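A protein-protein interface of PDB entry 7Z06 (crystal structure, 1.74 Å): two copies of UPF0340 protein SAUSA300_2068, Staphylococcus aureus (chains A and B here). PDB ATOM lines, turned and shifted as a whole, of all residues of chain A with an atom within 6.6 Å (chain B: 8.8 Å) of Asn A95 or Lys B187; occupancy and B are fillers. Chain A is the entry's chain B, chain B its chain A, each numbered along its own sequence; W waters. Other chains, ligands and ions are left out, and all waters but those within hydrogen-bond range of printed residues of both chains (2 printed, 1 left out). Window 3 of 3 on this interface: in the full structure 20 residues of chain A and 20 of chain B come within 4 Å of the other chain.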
ATOM      1  N   GLY A  90     -14.707 -28.364  -6.152  1.00  0.00           N
ATOM      2  CA  GLY A  90     -15.418 -28.663  -7.403  1.00  0.00           C
ATOM      3  C   GLY A  90     -14.994 -30.017  -7.927  1.00  0.00           C
ATOM      4  O   GLY A  90     -14.047 -30.592  -7.372  1.00  0.00           O
ATOM      5  N   CYS A  91     -15.664 -30.499  -8.971  1.00  0.00           N
ATOM      6  CA  CYS A  91     -15.342 -31.830  -9.541  1.00  0.00           C
ATOM      7  C   CYS A  91     -14.051 -31.765 -10.363  1.00  0.00           C
ATOM      8  O   CYS A  91     -13.490 -30.664 -10.495  1.00  0.00           O
ATOM      9  CB  CYS A  91     -16.489 -32.342 -10.404  1.00  0.00           C
ATOM     10  SG  CYS A  91     -16.752 -31.383 -11.918  1.00  0.00           S
ATOM     11  N   GLU A  92     -13.614 -32.904 -10.895  1.00  0.00           N
ATOM     12  CA  GLU A  92     -12.332 -32.974 -11.643  1.00  0.00           C
ATOM     13  C   GLU A  92     -12.400 -32.200 -12.970  1.00  0.00           C
ATOM     14  O   GLU A  92     -11.332 -31.841 -13.484  1.00  0.00           O
ATOM     15  CB  GLU A  92     -11.959 -34.433 -11.900  1.00  0.00           C
ATOM     16  CG  GLU A  92     -12.223 -35.349 -10.720  1.00  0.00           C
ATOM     17  CD  GLU A  92     -13.646 -35.876 -10.643  1.00  0.00           C
ATOM     18  OE1 GLU A  92     -13.997 -36.746 -11.463  1.00  0.00           O
ATOM     19  OE2 GLU A  92     -14.400 -35.409  -9.770  1.00  0.00           O
ATOM     20  N   HIS A  93     -13.603 -31.970 -13.508  1.00  0.00           N
ATOM     21  CA  HIS A  93     -13.739 -31.197 -14.774  1.00  0.00           C
ATOM     22  C   HIS A  93     -13.205 -29.775 -14.564  1.00  0.00           C
ATOM     23  O   HIS A  93     -12.719 -29.186 -15.544  1.00  0.00           O
ATOM     24  CB  HIS A  93     -15.179 -31.209 -15.303  1.00  0.00           C
ATOM     25  CG  HIS A  93     -15.283 -30.778 -16.727  1.00  0.00           C
ATOM     26  ND1 HIS A  93     -14.888 -31.587 -17.772  1.00  0.00           N
ATOM     27  CD2 HIS A  93     -15.726 -29.630 -17.284  1.00  0.00           C
ATOM     28  CE1 HIS A  93     -15.085 -30.958 -18.912  1.00  0.00           C
ATOM     29  NE2 HIS A  93     -15.599 -29.757 -18.639  1.00  0.00           N
ATOM     30  N   ILE A  94     -13.316 -29.243 -13.345  1.00  0.00           N
ATOM     31  CA  ILE A  94     -12.722 -27.909 -13.033  1.00  0.00           C
ATOM     32  C   ILE A  94     -11.485 -28.128 -12.146  1.00  0.00           C
ATOM     33  O   ILE A  94     -11.199 -27.251 -11.318  1.00  0.00           O
ATOM     34  CB  ILE A  94     -13.756 -26.941 -12.427  1.00  0.00           C
ATOM     35  CG1 ILE A  94     -14.320 -27.445 -11.097  1.00  0.00           C
ATOM     36  CG2 ILE A  94     -14.861 -26.645 -13.432  1.00  0.00           C
ATOM     37  CD1 ILE A  94     -15.174 -26.427 -10.383  1.00  0.00           C
ATOM     38  N   ASN A  95     -10.815 -29.270 -12.299  1.00  0.00           N
ATOM     39  CA  ASN A  95      -9.523 -29.524 -11.598  1.00  0.00           C
ATOM     40  C   ASN A  95      -9.647 -29.431 -10.069  1.00  0.00           C
ATOM     41  O   ASN A  95      -8.652 -29.067  -9.430  1.00  0.00           O
ATOM     42  CB  ASN A  95      -8.441 -28.568 -12.106  1.00  0.00           C
ATOM     43  CG  ASN A  95      -8.347 -28.543 -13.618  1.00  0.00           C
ATOM     44  OD1 ASN A  95      -8.642 -29.535 -14.279  1.00  0.00           O
ATOM     45  ND2 ASN A  95      -7.930 -27.417 -14.170  1.00  0.00           N
ATOM     46  N   ARG A  96     -10.811 -29.772  -9.515  1.00  0.00           N
ATOM     47  CA  ARG A  96     -11.015 -29.723  -8.043  1.00  0.00           C
ATOM     48  C   ARG A  96     -10.760 -28.300  -7.541  1.00  0.00           C
ATOM     49  O   ARG A  96     -10.379 -28.150  -6.369  1.00  0.00           O
ATOM     50  CB  ARG A  96     -10.106 -30.736  -7.343  1.00  0.00           C
ATOM     51  CG  ARG A  96     -10.463 -32.192  -7.606  1.00  0.00           C
ATOM     52  CD  ARG A  96      -9.494 -33.119  -6.898  1.00  0.00           C
ATOM     53  NE  ARG A  96      -9.797 -34.529  -7.091  1.00  0.00           N
ATOM     54  CZ  ARG A  96     -10.520 -35.266  -6.256  1.00  0.00           C
ATOM     55  NH1 ARG A  96     -11.020 -34.726  -5.159  1.00  0.00           N
ATOM     56  NH2 ARG A  96     -10.737 -36.541  -6.522  1.00  0.00           N
ATOM     57  N   ALA A  97     -10.972 -27.300  -8.400  1.00  0.00           N
ATOM     58  CA  ALA A  97     -10.820 -25.892  -7.974  1.00  0.00           C
ATOM     59  C   ALA A  97     -11.770 -25.637  -6.808  1.00  0.00           C
ATOM     60  O   ALA A  97     -12.821 -26.298  -6.752  1.00  0.00           O
ATOM     61  CB  ALA A  97     -11.086 -24.958  -9.125  1.00  0.00           C
ATOM     62  N   ILE A  98     -11.432 -24.691  -5.935  1.00  0.00           N
ATOM     63  CA  ILE A  98     -12.250 -24.514  -4.703  1.00  0.00           C
ATOM     64  C   ILE A  98     -12.999 -23.186  -4.693  1.00  0.00           C
ATOM     65  O   ILE A  98     -12.369 -22.145  -4.932  1.00  0.00           O
ATOM     66  CB  ILE A  98     -11.373 -24.670  -3.439  1.00  0.00           C
ATOM     67  CG1 ILE A  98     -10.612 -25.998  -3.429  1.00  0.00           C
ATOM     68  CG2 ILE A  98     -12.204 -24.486  -2.180  1.00  0.00           C
ATOM     69  CD1 ILE A  98      -9.271 -25.946  -4.122  1.00  0.00           C
ATOM     70  N   GLU A 140      -7.262 -22.206  -7.115  1.00  0.00           N
ATOM     71  CA  GLU A 140      -6.731 -23.417  -7.709  1.00  0.00           C
ATOM     72  C   GLU A 140      -6.499 -24.545  -6.716  1.00  0.00           C
ATOM     73  O   GLU A 140      -6.726 -25.727  -7.019  1.00  0.00           O
ATOM     74  CB  GLU A 140      -5.476 -23.146  -8.505  1.00  0.00           C
ATOM     75  CG  GLU A 140      -5.207 -24.242  -9.539  1.00  0.00           C
ATOM     76  CD  GLU A 140      -4.248 -23.872 -10.626  1.00  0.00           C
ATOM     77  OE1 GLU A 140      -3.274 -23.137 -10.319  1.00  0.00           O
ATOM     78  OE2 GLU A 140      -4.485 -24.312 -11.784  1.00  0.00           O
ATOM     79  N   HIS A 141      -6.055 -24.156  -5.522  1.00  0.00           N
ATOM     80  CA  HIS A 141      -5.616 -25.068  -4.464  1.00  0.00           C
ATOM     81  C   HIS A 141      -5.922 -24.407  -3.136  1.00  0.00           C
ATOM     82  O   HIS A 141      -5.979 -23.171  -3.032  1.00  0.00           O
ATOM     83  CB  HIS A 141      -4.094 -25.313  -4.506  1.00  0.00           C
ATOM     84  CG  HIS A 141      -3.603 -25.960  -5.768  1.00  0.00           C
ATOM     85  ND1 HIS A 141      -3.814 -27.292  -6.048  1.00  0.00           N
ATOM     86  CD2 HIS A 141      -2.916 -25.465  -6.824  1.00  0.00           C
ATOM     87  CE1 HIS A 141      -3.276 -27.594  -7.207  1.00  0.00           C
ATOM     88  NE2 HIS A 141      -2.727 -26.500  -7.710  1.00  0.00           N
ATOM     89  N   HIS A 158      -6.373 -31.452   0.264  1.00  0.00           N
ATOM     90  CA  HIS A 158      -6.646 -30.119   0.810  1.00  0.00           C
ATOM     91  C   HIS A 158      -6.385 -29.912   2.292  1.00  0.00           C
ATOM     92  O   HIS A 158      -6.530 -28.804   2.793  1.00  0.00           O
ATOM     93  CB  HIS A 158      -8.091 -29.722   0.546  1.00  0.00           C
ATOM     94  CG  HIS A 158      -8.516 -29.904  -0.875  1.00  0.00           C
ATOM     95  ND1 HIS A 158      -7.937 -29.189  -1.906  1.00  0.00           N
ATOM     96  CD2 HIS A 158      -9.476 -30.680  -1.437  1.00  0.00           C
ATOM     97  CE1 HIS A 158      -8.530 -29.513  -3.042  1.00  0.00           C
ATOM     98  NE2 HIS A 158      -9.448 -30.429  -2.798  1.00  0.00           N
ATOM     99  N   HIS B 161      -1.837 -34.103  -8.827  1.00  0.00           N
ATOM    100  CA  HIS B 161      -2.970 -33.279  -9.270  1.00  0.00           C
ATOM    101  C   HIS B 161      -3.118 -33.484 -10.768  1.00  0.00           C
ATOM    102  O   HIS B 161      -2.124 -33.435 -11.486  1.00  0.00           O
ATOM    103  CB  HIS B 161      -2.666 -31.834  -8.932  1.00  0.00           C
ATOM    104  CG  HIS B 161      -3.823 -30.911  -9.056  1.00  0.00           C
ATOM    105  ND1 HIS B 161      -4.967 -31.051  -8.299  1.00  0.00           N
ATOM    106  CD2 HIS B 161      -4.001 -29.801  -9.807  1.00  0.00           C
ATOM    107  CE1 HIS B 161      -5.788 -30.063  -8.563  1.00  0.00           C
ATOM    108  NE2 HIS B 161      -5.230 -29.284  -9.476  1.00  0.00           N
ATOM    109  N   VAL B 162      -4.327 -33.764 -11.282  1.00  0.00           N
ATOM    110  CA  VAL B 162      -5.606 -33.751 -10.605  1.00  0.00           C
ATOM    111  C   VAL B 162      -6.010 -35.203 -10.286  1.00  0.00           C
ATOM    112  O   VAL B 162      -5.994 -36.092 -11.145  1.00  0.00           O
ATOM    113  CB  VAL B 162      -6.713 -33.194 -11.557  1.00  0.00           C
ATOM    114  CG1 VAL B 162      -8.077 -33.233 -10.901  1.00  0.00           C
ATOM    115  CG2 VAL B 162      -6.394 -31.776 -12.003  1.00  0.00           C
ATOM    116  N   CYS B 163      -6.398 -35.428  -9.043  1.00  0.00           N
ATOM    117  CA  CYS B 163      -6.774 -36.746  -8.560  1.00  0.00           C
ATOM    118  C   CYS B 163      -8.208 -37.074  -9.022  1.00  0.00           C
ATOM    119  O   CYS B 163      -9.125 -36.256  -8.845  1.00  0.00           O
ATOM    120  CB  CYS B 163      -6.699 -36.731  -7.055  1.00  0.00           C
ATOM    121  SG  CYS B 163      -7.327 -38.221  -6.227  1.00  0.00           S
ATOM    122  N   VAL B 164      -8.376 -38.251  -9.627  1.00  0.00           N
ATOM    123  CA  VAL B 164      -9.668 -38.708 -10.182  1.00  0.00           C
ATOM    124  C   VAL B 164     -10.029 -40.049  -9.556  1.00  0.00           C
ATOM    125  O   VAL B 164      -9.324 -41.022  -9.758  1.00  0.00           O
ATOM    126  CB  VAL B 164      -9.600 -38.872 -11.713  1.00  0.00           C
ATOM    127  CG1 VAL B 164     -10.961 -39.254 -12.299  1.00  0.00           C
ATOM    128  CG2 VAL B 164      -9.051 -37.594 -12.361  1.00  0.00           C
ATOM    129  N   ARG B 184      -4.763 -37.227 -13.688  1.00  0.00           N
ATOM    130  CA  ARG B 184      -4.772 -36.693 -15.072  1.00  0.00           C
ATOM    131  C   ARG B 184      -4.393 -35.218 -15.017  1.00  0.00           C
ATOM    132  O   ARG B 184      -4.561 -34.544 -14.004  1.00  0.00           O
ATOM    133  CB  ARG B 184      -6.142 -36.890 -15.718  1.00  0.00           C
ATOM    134  CG  ARG B 184      -7.199 -35.957 -15.161  1.00  0.00           C
ATOM    135  CD  ARG B 184      -8.532 -36.188 -15.858  1.00  0.00           C
ATOM    136  NE  ARG B 184      -9.456 -35.145 -15.452  1.00  0.00           N
ATOM    137  CZ  ARG B 184     -10.754 -35.170 -15.626  1.00  0.00           C
ATOM    138  NH1 ARG B 184     -11.345 -36.232 -16.146  1.00  0.00           N
ATOM    139  NH2 ARG B 184     -11.470 -34.123 -15.267  1.00  0.00           N
ATOM    140  N   PRO B 185      -3.901 -34.646 -16.127  1.00  0.00           N
ATOM    141  CA  PRO B 185      -3.504 -33.235 -16.118  1.00  0.00           C
ATOM    142  C   PRO B 185      -4.674 -32.275 -15.860  1.00  0.00           C
ATOM    143  O   PRO B 185      -5.817 -32.607 -16.199  1.00  0.00           O
ATOM    144  CB  PRO B 185      -2.934 -33.048 -17.521  1.00  0.00           C
ATOM    145  CG  PRO B 185      -2.482 -34.436 -17.926  1.00  0.00           C
ATOM    146  CD  PRO B 185      -3.536 -35.353 -17.355  1.00  0.00           C
ATOM    147  N   LYS B 186      -4.377 -31.103 -15.307  1.00  0.00           N
ATOM    148  CA  LYS B 186      -5.348 -30.006 -15.254  1.00  0.00           C
ATOM    149  C   LYS B 186      -5.819 -29.677 -16.665  1.00  0.00           C
ATOM    150  O   LYS B 186      -5.036 -29.654 -17.594  1.00  0.00           O
ATOM    151  CB  LYS B 186      -4.721 -28.749 -14.623  1.00  0.00           C
ATOM    152  CG  LYS B 186      -4.396 -28.843 -13.187  1.00  0.00           C
ATOM    153  CD  LYS B 186      -3.874 -27.545 -12.577  1.00  0.00           C
ATOM    154  CE  LYS B 186      -2.731 -26.890 -13.333  1.00  0.00           C
ATOM    155  NZ  LYS B 186      -2.076 -25.877 -12.456  1.00  0.00           N
ATOM    156  N   LYS B 187      -7.134 -29.467 -16.819  1.00  0.00           N
ATOM    157  CA  LYS B 187      -7.695 -28.933 -18.052  1.00  0.00           C
ATOM    158  C   LYS B 187      -7.661 -27.418 -17.970  1.00  0.00           C
ATOM    159  O   LYS B 187      -8.127 -26.819 -16.994  1.00  0.00           O
ATOM    160  CB  LYS B 187      -9.121 -29.465 -18.249  1.00  0.00           C
ATOM    161  CG  LYS B 187      -9.101 -30.971 -18.531  1.00  0.00           C
ATOM    162  CD  LYS B 187     -10.489 -31.562 -18.584  1.00  0.00           C
ATOM    163  CE  LYS B 187     -10.452 -33.084 -18.491  1.00  0.00           C
ATOM    164  NZ  LYS B 187      -9.536 -33.704 -19.484  1.00  0.00           N
ATOM    165  N   ILE B 188      -7.124 -26.775 -19.018  1.00  0.00           N
ATOM    166  CA  ILE B 188      -6.986 -25.339 -18.973  1.00  0.00           C
ATOM    167  C   ILE B 188      -7.560 -24.715 -20.246  1.00  0.00           C
ATOM    168  O   ILE B 188      -7.765 -25.372 -21.249  1.00  0.00           O
ATOM    169  CB  ILE B 188      -5.514 -24.913 -18.760  1.00  0.00           C
ATOM    170  CG1 ILE B 188      -4.681 -25.391 -19.960  1.00  0.00           C
ATOM    171  CG2 ILE B 188      -4.946 -25.450 -17.454  1.00  0.00           C
ATOM    172  CD1 ILE B 188      -3.797 -24.314 -20.541  1.00  0.00           C
ATOM    173  N   GLY B 189      -7.841 -23.420 -20.155  1.00  0.00           N
ATOM    174  CA  GLY B 189      -8.260 -22.624 -21.301  1.00  0.00           C
ATOM    175  C   GLY B 189      -9.673 -22.133 -21.085  1.00  0.00           C
ATOM    176  O   GLY B 189     -10.449 -22.701 -20.259  1.00  0.00           O
ATOM    177  N   GLY B 190     -10.016 -21.076 -21.815  1.00  0.00           N
ATOM    178  CA  GLY B 190     -11.337 -20.483 -21.817  1.00  0.00           C
ATOM    179  C   GLY B 190     -12.381 -21.192 -22.632  1.00  0.00           C
ATOM    180  O   GLY B 190     -12.202 -22.310 -23.096  1.00  0.00           O
ATOM    181  N   ALA B 193     -11.508 -22.884 -25.998  1.00  0.00           N
ATOM    182  CA  ALA B 193     -10.476 -23.903 -26.016  1.00  0.00           C
ATOM    183  C   ALA B 193     -10.994 -25.262 -26.458  1.00  0.00           C
ATOM    184  O   ALA B 193     -12.186 -25.592 -26.254  1.00  0.00           O
ATOM    185  CB  ALA B 193      -9.788 -24.000 -24.673  1.00  0.00           C
ATOM    186  N   LYS B 194     -10.110 -26.021 -27.118  1.00  0.00           N
ATOM    187  CA  LYS B 194     -10.365 -27.359 -27.611  1.00  0.00           C
ATOM    188  C   LYS B 194      -9.568 -28.368 -26.846  1.00  0.00           C
ATOM    189  O   LYS B 194      -8.524 -28.046 -26.330  1.00  0.00           O
ATOM    190  CB  LYS B 194      -9.989 -27.421 -29.105  1.00  0.00           C
ATOM    191  CG  LYS B 194     -10.789 -26.494 -29.986  1.00  0.00           C
ATOM    192  CD  LYS B 194     -12.178 -27.073 -30.202  1.00  0.00           C
ATOM    193  CE  LYS B 194     -13.127 -26.089 -30.888  1.00  0.00           C
ATOM    194  NZ  LYS B 194     -13.215 -24.930 -29.917  1.00  0.00           N
ATOM    195  N   TYR B 195     -10.084 -29.605 -26.747  1.00  0.00           N
ATOM    196  CA  TYR B 195      -9.467 -30.711 -25.952  1.00  0.00           C
ATOM    197  C   TYR B 195      -9.272 -31.957 -26.835  1.00  0.00           C
ATOM    198  O   TYR B 195      -8.754 -32.971 -26.345  1.00  0.00           O
ATOM    199  CB  TYR B 195     -10.252 -30.915 -24.645  1.00  0.00           C
ATOM    200  CG  TYR B 195     -10.329 -29.637 -23.856  1.00  0.00           C
ATOM    201  CD1 TYR B 195      -9.278 -29.246 -23.051  1.00  0.00           C
ATOM    202  CD2 TYR B 195     -11.350 -28.723 -24.066  1.00  0.00           C
ATOM    203  CE1 TYR B 195      -9.289 -28.025 -22.394  1.00  0.00           C
ATOM    204  CE2 TYR B 195     -11.380 -27.501 -23.413  1.00  0.00           C
ATOM    205  CZ  TYR B 195     -10.322 -27.130 -22.615  1.00  0.00           C
ATOM    206  OH  TYR B 195     -10.365 -25.915 -22.005  1.00  0.00           O
HETATM  207  O   HOH W   1      -7.157 -26.871  -9.546  1.00  0.00           O
HETATM  208  O   HOH W   2      -1.110 -26.730  -9.905  1.00  0.00           O
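O of Cys B163 is in hydrogen-bond range of NE of Arg A96, at 2.6 Å. The guanidinium group (NH2) of Arg B184 sits at hydrogen-bond distance from the backbone carbonyl oxygen (O) of Glu A92, 2.9 Å away. The side-chain amino group of Lys B186 lies within salt-bridge range of the side-chain carboxylate of Glu A140. The backbone carbonyl oxygen of Asn A95 lies close to a ring nitrogen (NE2) of His B161 (3.4 Å). ND2 of Asn A95 lies within hydrogen-bond range of O of Lys B187 (2.9 Å).
The side-chain sulfur (SG) of Cys A91 lies close to the backbone NH (N) of His A93 (3.6 Å). The backbone carbonyl oxygen of Arg B184 is in hydrogen-bond range of the backbone NH of Val B162. The backbone NH (N) of Arg A96 lies within hydrogen-bond range of the backbone carbonyl oxygen (O) of Cys A91.
O of Cys B163 touches CG of Glu A92 (3.7 Å). Arg B184 touches His A93 (NH2 to N, 3.5 Å). CB of Asn A95 touches CG2 of Val B162, at 3.8 Å. Asn A95 touches Lys B186 (OD1 to CA, 3.5 Å). His A141 touches His B161.
Of the printed residues of chain B, His A93 touches Arg B184. Of chain B, only His B161, Val B162, Lys B186 and Lys B187 come within 4 Å of Asn A95. Printed residues of chain A within 4 Å of His B161: Asn A95 (3.2 Å) and His A141 (3.4 Å). Of the printed residues of chain A, Cys B163 touches Glu A92 (3.7 Å) and Arg A96 (2.6 Å). Val B164 touches none of the printed residues of chain A. Lys B187 touches just one residue of chain A: Asn A95 (2.9 Å). The nearest residue of chain A that does not touch Lys B187 is His A93 (4.5 Å).
Of the 14 printed residues of chain B, 6 touch a printed residue of chain A. Among the printed residues, 10 pairs touch across the chains.
No position is printed for both chains. Of the 10 pairs that touch across the chains among the printed residues, none has its exchanged pair printed and touching as well.
Water W1 lies within hydrogen-bond range of O of Asn A95 (2.7 Å), O of Glu A140 (2.8 Å) and NE2 of His B161 (3.1 Å). Water W2 lies within hydrogen-bond range of a ring nitrogen (NE2) of His A141 and the side-chain amino group of Lys B186.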
